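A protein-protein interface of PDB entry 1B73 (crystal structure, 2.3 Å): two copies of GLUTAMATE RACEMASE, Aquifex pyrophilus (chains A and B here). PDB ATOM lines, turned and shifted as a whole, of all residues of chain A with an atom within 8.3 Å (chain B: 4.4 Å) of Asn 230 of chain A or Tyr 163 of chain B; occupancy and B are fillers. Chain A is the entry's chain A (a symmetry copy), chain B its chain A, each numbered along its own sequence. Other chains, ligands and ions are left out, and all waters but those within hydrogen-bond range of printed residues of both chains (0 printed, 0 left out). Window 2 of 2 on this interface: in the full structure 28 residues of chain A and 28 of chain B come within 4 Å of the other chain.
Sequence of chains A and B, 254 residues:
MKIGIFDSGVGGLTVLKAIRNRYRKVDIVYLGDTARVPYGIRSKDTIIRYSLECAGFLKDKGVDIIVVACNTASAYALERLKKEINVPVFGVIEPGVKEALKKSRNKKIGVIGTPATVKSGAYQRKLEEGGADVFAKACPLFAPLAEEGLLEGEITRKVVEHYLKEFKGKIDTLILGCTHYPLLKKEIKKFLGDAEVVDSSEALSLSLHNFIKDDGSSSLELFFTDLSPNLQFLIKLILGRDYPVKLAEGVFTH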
ATOM      1  N   VAL A  10      -4.001 -32.723  -2.086  1.00  0.00           N
ATOM      2  CA  VAL A  10      -3.592 -33.550  -3.224  1.00  0.00           C
ATOM      3  C   VAL A  10      -2.877 -34.810  -2.777  1.00  0.00           C
ATOM      4  O   VAL A  10      -2.399 -35.572  -3.622  1.00  0.00           O
ATOM      5  CB  VAL A  10      -2.621 -32.781  -4.163  1.00  0.00           C
ATOM      6  CG1 VAL A  10      -3.284 -31.470  -4.610  1.00  0.00           C
ATOM      7  CG2 VAL A  10      -1.321 -32.428  -3.436  1.00  0.00           C
ATOM      8  N   LEU A 227      -9.606 -23.556  -6.498  1.00  0.00           N
ATOM      9  CA  LEU A 227      -8.591 -23.652  -7.534  1.00  0.00           C
ATOM     10  C   LEU A 227      -7.308 -22.953  -7.029  1.00  0.00           C
ATOM     11  O   LEU A 227      -6.770 -22.032  -7.657  1.00  0.00           O
ATOM     12  CB  LEU A 227      -9.122 -23.004  -8.820  1.00  0.00           C
ATOM     13  CG  LEU A 227      -9.694 -23.927  -9.906  1.00  0.00           C
ATOM     14  CD1 LEU A 227      -8.866 -25.217  -9.945  1.00  0.00           C
ATOM     15  CD2 LEU A 227     -11.129 -24.265  -9.700  1.00  0.00           C
ATOM     16  N   SER A 228      -6.848 -23.409  -5.863  1.00  0.00           N
ATOM     17  CA  SER A 228      -5.673 -22.901  -5.178  1.00  0.00           C
ATOM     18  C   SER A 228      -4.496 -22.669  -6.133  1.00  0.00           C
ATOM     19  O   SER A 228      -4.530 -23.093  -7.292  1.00  0.00           O
ATOM     20  CB  SER A 228      -5.297 -23.889  -4.064  1.00  0.00           C
ATOM     21  OG  SER A 228      -6.383 -24.073  -3.155  1.00  0.00           O
ATOM     22  N   PRO A 229      -3.463 -21.950  -5.667  1.00  0.00           N
ATOM     23  CA  PRO A 229      -2.265 -21.640  -6.456  1.00  0.00           C
ATOM     24  C   PRO A 229      -1.729 -22.740  -7.374  1.00  0.00           C
ATOM     25  O   PRO A 229      -2.287 -22.977  -8.444  1.00  0.00           O
ATOM     26  CB  PRO A 229      -1.236 -21.227  -5.391  1.00  0.00           C
ATOM     27  CG  PRO A 229      -1.913 -21.556  -4.041  1.00  0.00           C
ATOM     28  CD  PRO A 229      -3.359 -21.333  -4.338  1.00  0.00           C
ATOM     29  N   ASN A 230      -0.678 -23.420  -6.923  1.00  0.00           N
ATOM     30  CA  ASN A 230      -0.002 -24.461  -7.690  1.00  0.00           C
ATOM     31  C   ASN A 230      -0.654 -25.823  -7.747  1.00  0.00           C
ATOM     32  O   ASN A 230       0.024 -26.819  -8.012  1.00  0.00           O
ATOM     33  CB  ASN A 230       1.441 -24.628  -7.195  1.00  0.00           C
ATOM     34  CG  ASN A 230       1.989 -23.368  -6.568  1.00  0.00           C
ATOM     35  OD1 ASN A 230       2.612 -22.560  -7.234  1.00  0.00           O
ATOM     36  ND2 ASN A 230       1.765 -23.206  -5.269  1.00  0.00           N
ATOM     37  N   LEU A 231      -1.945 -25.878  -7.439  1.00  0.00           N
ATOM     38  CA  LEU A 231      -2.737 -27.106  -7.489  1.00  0.00           C
ATOM     39  C   LEU A 231      -2.391 -27.802  -8.799  1.00  0.00           C
ATOM     40  O   LEU A 231      -1.654 -28.784  -8.831  1.00  0.00           O
ATOM     41  CB  LEU A 231      -4.221 -26.740  -7.547  1.00  0.00           C
ATOM     42  CG  LEU A 231      -5.337 -27.785  -7.387  1.00  0.00           C
ATOM     43  CD1 LEU A 231      -6.088 -27.398  -6.158  1.00  0.00           C
ATOM     44  CD2 LEU A 231      -6.294 -27.730  -8.575  1.00  0.00           C
ATOM     45  N   GLN A 232      -2.798 -27.157  -9.884  1.00  0.00           N
ATOM     46  CA  GLN A 232      -2.611 -27.616 -11.246  1.00  0.00           C
ATOM     47  C   GLN A 232      -1.220 -28.155 -11.562  1.00  0.00           C
ATOM     48  O   GLN A 232      -1.080 -29.115 -12.328  1.00  0.00           O
ATOM     49  CB  GLN A 232      -2.975 -26.470 -12.210  1.00  0.00           C
ATOM     50  CG  GLN A 232      -3.953 -25.396 -11.653  1.00  0.00           C
ATOM     51  CD  GLN A 232      -3.275 -24.306 -10.799  1.00  0.00           C
ATOM     52  OE1 GLN A 232      -2.059 -24.342 -10.552  1.00  0.00           O
ATOM     53  NE2 GLN A 232      -4.065 -23.317 -10.368  1.00  0.00           N
ATOM     54  N   PHE A 233      -0.191 -27.518 -11.001  1.00  0.00           N
ATOM     55  CA  PHE A 233       1.214 -27.912 -11.209  1.00  0.00           C
ATOM     56  C   PHE A 233       1.536 -29.245 -10.475  1.00  0.00           C
ATOM     57  O   PHE A 233       2.247 -30.145 -10.982  1.00  0.00           O
ATOM     58  CB  PHE A 233       2.098 -26.778 -10.666  1.00  0.00           C
ATOM     59  CG  PHE A 233       3.564 -27.079 -10.700  1.00  0.00           C
ATOM     60  CD1 PHE A 233       4.317 -27.059  -9.545  1.00  0.00           C
ATOM     61  CD2 PHE A 233       4.170 -27.458 -11.898  1.00  0.00           C
ATOM     62  CE1 PHE A 233       5.670 -27.432  -9.575  1.00  0.00           C
ATOM     63  CE2 PHE A 233       5.509 -27.825 -11.931  1.00  0.00           C
ATOM     64  CZ  PHE A 233       6.258 -27.817 -10.764  1.00  0.00           C
ATOM     65  N   LEU A 234       1.049 -29.318  -9.243  1.00  0.00           N
ATOM     66  CA  LEU A 234       1.210 -30.479  -8.362  1.00  0.00           C
ATOM     67  C   LEU A 234       0.572 -31.711  -8.981  1.00  0.00           C
ATOM     68  O   LEU A 234       1.133 -32.817  -8.948  1.00  0.00           O
ATOM     69  CB  LEU A 234       0.568 -30.195  -6.998  1.00  0.00           C
ATOM     70  CG  LEU A 234       1.416 -29.244  -6.170  1.00  0.00           C
ATOM     71  CD1 LEU A 234       0.655 -28.696  -4.891  1.00  0.00           C
ATOM     72  CD2 LEU A 234       2.699 -29.981  -5.796  1.00  0.00           C
ATOM     73  N   ILE A 235      -0.603 -31.503  -9.554  1.00  0.00           N
ATOM     74  CA  ILE A 235      -1.379 -32.550 -10.233  1.00  0.00           C
ATOM     75  C   ILE A 235      -0.542 -33.165 -11.327  1.00  0.00           C
ATOM     76  O   ILE A 235      -0.469 -34.392 -11.441  1.00  0.00           O
ATOM     77  CB  ILE A 235      -2.602 -31.921 -10.871  1.00  0.00           C
ATOM     78  CG1 ILE A 235      -3.654 -31.686  -9.813  1.00  0.00           C
ATOM     79  CG2 ILE A 235      -3.127 -32.747 -12.038  1.00  0.00           C
ATOM     80  CD1 ILE A 235      -5.007 -31.865 -10.376  1.00  0.00           C
ATOM     81  N   LYS A 236       0.100 -32.277 -12.092  1.00  0.00           N
ATOM     82  CA  LYS A 236       0.992 -32.584 -13.212  1.00  0.00           C
ATOM     83  C   LYS A 236       2.163 -33.480 -12.788  1.00  0.00           C
ATOM     84  O   LYS A 236       2.450 -34.462 -13.458  1.00  0.00           O
ATOM     85  CB  LYS A 236       1.546 -31.275 -13.798  1.00  0.00           C
ATOM     86  CG  LYS A 236       2.260 -31.426 -15.166  1.00  0.00           C
ATOM     87  CD  LYS A 236       3.360 -30.394 -15.367  1.00  0.00           C
ATOM     88  CE  LYS A 236       4.607 -30.776 -14.552  1.00  0.00           C
ATOM     89  NZ  LYS A 236       5.640 -29.694 -14.490  1.00  0.00           N
ATOM     90  N   LEU A 237       2.803 -33.125 -11.676  1.00  0.00           N
ATOM     91  CA  LEU A 237       3.949 -33.838 -11.102  1.00  0.00           C
ATOM     92  C   LEU A 237       3.608 -35.219 -10.495  1.00  0.00           C
ATOM     93  O   LEU A 237       4.401 -36.154 -10.603  1.00  0.00           O
ATOM     94  CB  LEU A 237       4.610 -32.965 -10.016  1.00  0.00           C
ATOM     95  CG  LEU A 237       5.253 -31.623 -10.419  1.00  0.00           C
ATOM     96  CD1 LEU A 237       5.216 -30.608  -9.282  1.00  0.00           C
ATOM     97  CD2 LEU A 237       6.689 -31.823 -10.882  1.00  0.00           C
ATOM     98  N   LYS B 137      12.067 -14.966  -8.587  1.00  0.00           N
ATOM     99  CA  LYS B 137      11.099 -16.090  -8.609  1.00  0.00           C
ATOM    100  C   LYS B 137      10.505 -16.210  -7.200  1.00  0.00           C
ATOM    101  O   LYS B 137      11.188 -15.915  -6.208  1.00  0.00           O
ATOM    102  CB  LYS B 137      11.765 -17.410  -9.037  1.00  0.00           C
ATOM    103  CG  LYS B 137      10.807 -18.578  -9.384  1.00  0.00           C
ATOM    104  CD  LYS B 137       9.552 -18.149 -10.180  1.00  0.00           C
ATOM    105  CE  LYS B 137       9.841 -17.641 -11.589  1.00  0.00           C
ATOM    106  NZ  LYS B 137       8.658 -16.960 -12.192  1.00  0.00           N
ATOM    107  N   ALA B 138       9.224 -16.559  -7.109  1.00  0.00           N
ATOM    108  CA  ALA B 138       8.523 -16.682  -5.820  1.00  0.00           C
ATOM    109  C   ALA B 138       8.620 -18.062  -5.137  1.00  0.00           C
ATOM    110  O   ALA B 138       8.899 -19.091  -5.765  1.00  0.00           O
ATOM    111  CB  ALA B 138       7.035 -16.281  -5.995  1.00  0.00           C
ATOM    112  N   PRO B 140       7.322 -21.379  -3.395  1.00  0.00           N
ATOM    113  CA  PRO B 140       6.132 -22.196  -3.704  1.00  0.00           C
ATOM    114  C   PRO B 140       5.438 -22.477  -2.372  1.00  0.00           C
ATOM    115  O   PRO B 140       6.083 -22.948  -1.436  1.00  0.00           O
ATOM    116  CB  PRO B 140       6.730 -23.481  -4.263  1.00  0.00           C
ATOM    117  CG  PRO B 140       8.000 -23.648  -3.471  1.00  0.00           C
ATOM    118  CD  PRO B 140       8.550 -22.198  -3.475  1.00  0.00           C
ATOM    119  N   LEU B 141       4.162 -22.115  -2.247  1.00  0.00           N
ATOM    120  CA  LEU B 141       3.442 -22.338  -0.995  1.00  0.00           C
ATOM    121  C   LEU B 141       2.843 -23.751  -1.028  1.00  0.00           C
ATOM    122  O   LEU B 141       1.699 -23.934  -1.431  1.00  0.00           O
ATOM    123  CB  LEU B 141       2.300 -21.314  -0.807  1.00  0.00           C
ATOM    124  CG  LEU B 141       2.125 -19.890  -1.387  1.00  0.00           C
ATOM    125  CD1 LEU B 141       3.097 -18.907  -0.770  1.00  0.00           C
ATOM    126  CD2 LEU B 141       2.182 -19.883  -2.903  1.00  0.00           C
ATOM    127  N   PHE B 142       3.577 -24.739  -0.537  1.00  0.00           N
ATOM    128  CA  PHE B 142       3.075 -26.099  -0.592  1.00  0.00           C
ATOM    129  C   PHE B 142       2.402 -26.782   0.589  1.00  0.00           C
ATOM    130  O   PHE B 142       1.388 -27.429   0.388  1.00  0.00           O
ATOM    131  CB  PHE B 142       4.142 -27.021  -1.190  1.00  0.00           C
ATOM    132  CG  PHE B 142       4.368 -26.821  -2.675  1.00  0.00           C
ATOM    133  CD1 PHE B 142       3.326 -26.476  -3.515  1.00  0.00           C
ATOM    134  CD2 PHE B 142       5.619 -27.042  -3.236  1.00  0.00           C
ATOM    135  CE1 PHE B 142       3.528 -26.361  -4.888  1.00  0.00           C
ATOM    136  CE2 PHE B 142       5.822 -26.931  -4.596  1.00  0.00           C
ATOM    137  CZ  PHE B 142       4.766 -26.589  -5.425  1.00  0.00           C
ATOM    138  N   VAL B 159      10.651 -30.044  -8.918  1.00  0.00           N
ATOM    139  CA  VAL B 159       9.983 -28.822  -8.540  1.00  0.00           C
ATOM    140  C   VAL B 159      11.073 -27.812  -8.799  1.00  0.00           C
ATOM    141  O   VAL B 159      10.964 -27.011  -9.726  1.00  0.00           O
ATOM    142  CB  VAL B 159       9.576 -28.832  -7.057  1.00  0.00           C
ATOM    143  CG1 VAL B 159       9.180 -27.462  -6.605  1.00  0.00           C
ATOM    144  CG2 VAL B 159       8.400 -29.770  -6.851  1.00  0.00           C
ATOM    145  N   VAL B 160      12.199 -28.040  -8.125  1.00  0.00           N
ATOM    146  CA  VAL B 160      13.393 -27.200  -8.197  1.00  0.00           C
ATOM    147  C   VAL B 160      13.697 -26.723  -9.622  1.00  0.00           C
ATOM    148  O   VAL B 160      13.389 -25.591  -9.964  1.00  0.00           O
ATOM    149  CB  VAL B 160      14.616 -27.946  -7.611  1.00  0.00           C
ATOM    150  CG1 VAL B 160      15.830 -27.044  -7.604  1.00  0.00           C
ATOM    151  CG2 VAL B 160      14.327 -28.418  -6.193  1.00  0.00           C
ATOM    152  N   GLU B 161      14.227 -27.617 -10.455  1.00  0.00           N
ATOM    153  CA  GLU B 161      14.568 -27.319 -11.844  1.00  0.00           C
ATOM    154  C   GLU B 161      13.533 -26.517 -12.618  1.00  0.00           C
ATOM    155  O   GLU B 161      13.885 -25.755 -13.508  1.00  0.00           O
ATOM    156  CB  GLU B 161      14.914 -28.612 -12.614  1.00  0.00           C
ATOM    157  CG  GLU B 161      16.108 -29.386 -12.043  1.00  0.00           C
ATOM    158  CD  GLU B 161      16.507 -30.608 -12.876  1.00  0.00           C
ATOM    159  OE1 GLU B 161      15.716 -31.586 -12.959  1.00  0.00           O
ATOM    160  OE2 GLU B 161      17.624 -30.596 -13.445  1.00  0.00           O
ATOM    161  N   HIS B 162      12.254 -26.690 -12.311  1.00  0.00           N
ATOM    162  CA  HIS B 162      11.225 -25.940 -13.033  1.00  0.00           C
ATOM    163  C   HIS B 162      11.121 -24.530 -12.473  1.00  0.00           C
ATOM    164  O   HIS B 162      10.754 -23.609 -13.183  1.00  0.00           O
ATOM    165  CB  HIS B 162       9.873 -26.653 -12.959  1.00  0.00           C
ATOM    166  CG  HIS B 162       8.780 -25.959 -13.707  1.00  0.00           C
ATOM    167  ND1 HIS B 162       7.899 -25.086 -13.108  1.00  0.00           N
ATOM    168  CD2 HIS B 162       8.410 -26.027 -15.010  1.00  0.00           C
ATOM    169  CE1 HIS B 162       7.038 -24.646 -13.996  1.00  0.00           C
ATOM    170  NE2 HIS B 162       7.321 -25.201 -15.167  1.00  0.00           N
ATOM    171  N   TYR B 163      11.413 -24.380 -11.185  1.00  0.00           N
ATOM    172  CA  TYR B 163      11.374 -23.081 -10.535  1.00  0.00           C
ATOM    173  C   TYR B 163      12.647 -22.320 -10.798  1.00  0.00           C
ATOM    174  O   TYR B 163      12.624 -21.157 -11.198  1.00  0.00           O
ATOM    175  CB  TYR B 163      11.195 -23.231  -9.036  1.00  0.00           C
ATOM    176  CG  TYR B 163       9.768 -23.191  -8.621  1.00  0.00           C
ATOM    177  CD1 TYR B 163       8.748 -23.450  -9.536  1.00  0.00           C
ATOM    178  CD2 TYR B 163       9.421 -22.895  -7.315  1.00  0.00           C
ATOM    179  CE1 TYR B 163       7.414 -23.412  -9.152  1.00  0.00           C
ATOM    180  CE2 TYR B 163       8.098 -22.860  -6.929  1.00  0.00           C
ATOM    181  CZ  TYR B 163       7.101 -23.122  -7.843  1.00  0.00           C
ATOM    182  OH  TYR B 163       5.795 -23.133  -7.425  1.00  0.00           O
ATOM    183  N   LEU B 164      13.764 -22.973 -10.525  1.00  0.00           N
ATOM    184  CA  LEU B 164      15.052 -22.364 -10.738  1.00  0.00           C
ATOM    185  C   LEU B 164      15.466 -22.672 -12.170  1.00  0.00           C
ATOM    186  O   LEU B 164      16.630 -22.954 -12.474  1.00  0.00           O
ATOM    187  CB  LEU B 164      16.040 -22.892  -9.693  1.00  0.00           C
ATOM    188  CG  LEU B 164      15.429 -22.705  -8.294  1.00  0.00           C
ATOM    189  CD1 LEU B 164      16.435 -22.884  -7.204  1.00  0.00           C
ATOM    190  CD2 LEU B 164      14.813 -21.400  -8.182  1.00  0.00           C
ATOM    191  N   LYS B 165      14.488 -22.573 -13.060  1.00  0.00           N
ATOM    192  CA  LYS B 165      14.714 -22.862 -14.475  1.00  0.00           C
ATOM    193  C   LYS B 165      15.569 -21.761 -15.105  1.00  0.00           C
ATOM    194  O   LYS B 165      16.767 -21.961 -15.373  1.00  0.00           O
ATOM    195  CB  LYS B 165      13.377 -23.001 -15.205  1.00  0.00           C
ATOM    196  CG  LYS B 165      13.508 -23.564 -16.592  1.00  0.00           C
ATOM    197  CD  LYS B 165      12.187 -23.563 -17.322  1.00  0.00           C
ATOM    198  CE  LYS B 165      12.369 -24.144 -18.715  1.00  0.00           C
ATOM    199  NZ  LYS B 165      11.068 -24.340 -19.391  1.00  0.00           N
ATOM    200  N   LEU B 183      12.494 -26.208  -1.753  1.00  0.00           N
ATOM    201  CA  LEU B 183      13.572 -25.301  -2.121  1.00  0.00           C
ATOM    202  C   LEU B 183      14.497 -24.991  -0.976  1.00  0.00           C
ATOM    203  O   LEU B 183      14.776 -23.831  -0.671  1.00  0.00           O
ATOM    204  CB  LEU B 183      13.022 -23.991  -2.701  1.00  0.00           C
ATOM    205  CG  LEU B 183      12.333 -24.080  -4.055  1.00  0.00           C
ATOM    206  CD1 LEU B 183      12.146 -22.671  -4.597  1.00  0.00           C
ATOM    207  CD2 LEU B 183      13.195 -24.897  -5.001  1.00  0.00           C
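Among the printed residues, merely in contact across the chains: Asn 230 of chain A with Leu 141 of chain B (3.9 Å), Asn 230 of chain A with Phe 142 of chain B (3.6 Å), Phe 233 of chain A with His 162 of chain B (3.8 Å) and Leu 234 of chain A with Phe 142 of chain B (3.7 Å).
OH of Tyr 163 of chain B lies within hydrogen-bond range of OD1 of Asn 230 of chain A (3.2 Å).
Among the printed residues, 5 pairs touch across the chains. Among the printed residues, no Asp or Glu carboxylate lies within 4 Å of a Lys or Arg side-chain nitrogen of the other chain.
Asn 230 of chain A touches just these residues of chain B: Leu 141 (3.9 Å), Phe 142 (3.6 Å) and Tyr 163 (3.2 Å). Of the printed residues of chain B, Leu 234 of chain A touches Phe 142 (3.7 Å). Lys 137 of chain B touches none of the printed residues of chain A. Of the printed residues of chain A, Phe 142 of chain B touches Asn 230 (3.6 Å) and Leu 234 (3.7 Å). Of the printed residues of chain A, His 162 of chain B touches Phe 233. Tyr 163 of chain B touches just one residue of chain A: Asn 230 (3.2 Å). Leu 183 of chain B touches none of the printed residues of chain A. The nearest printed residue of chain B that does not touch Asn 230 of chain A is Pro 140 of chain B (4.7 Å).
No position is printed for both chains.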
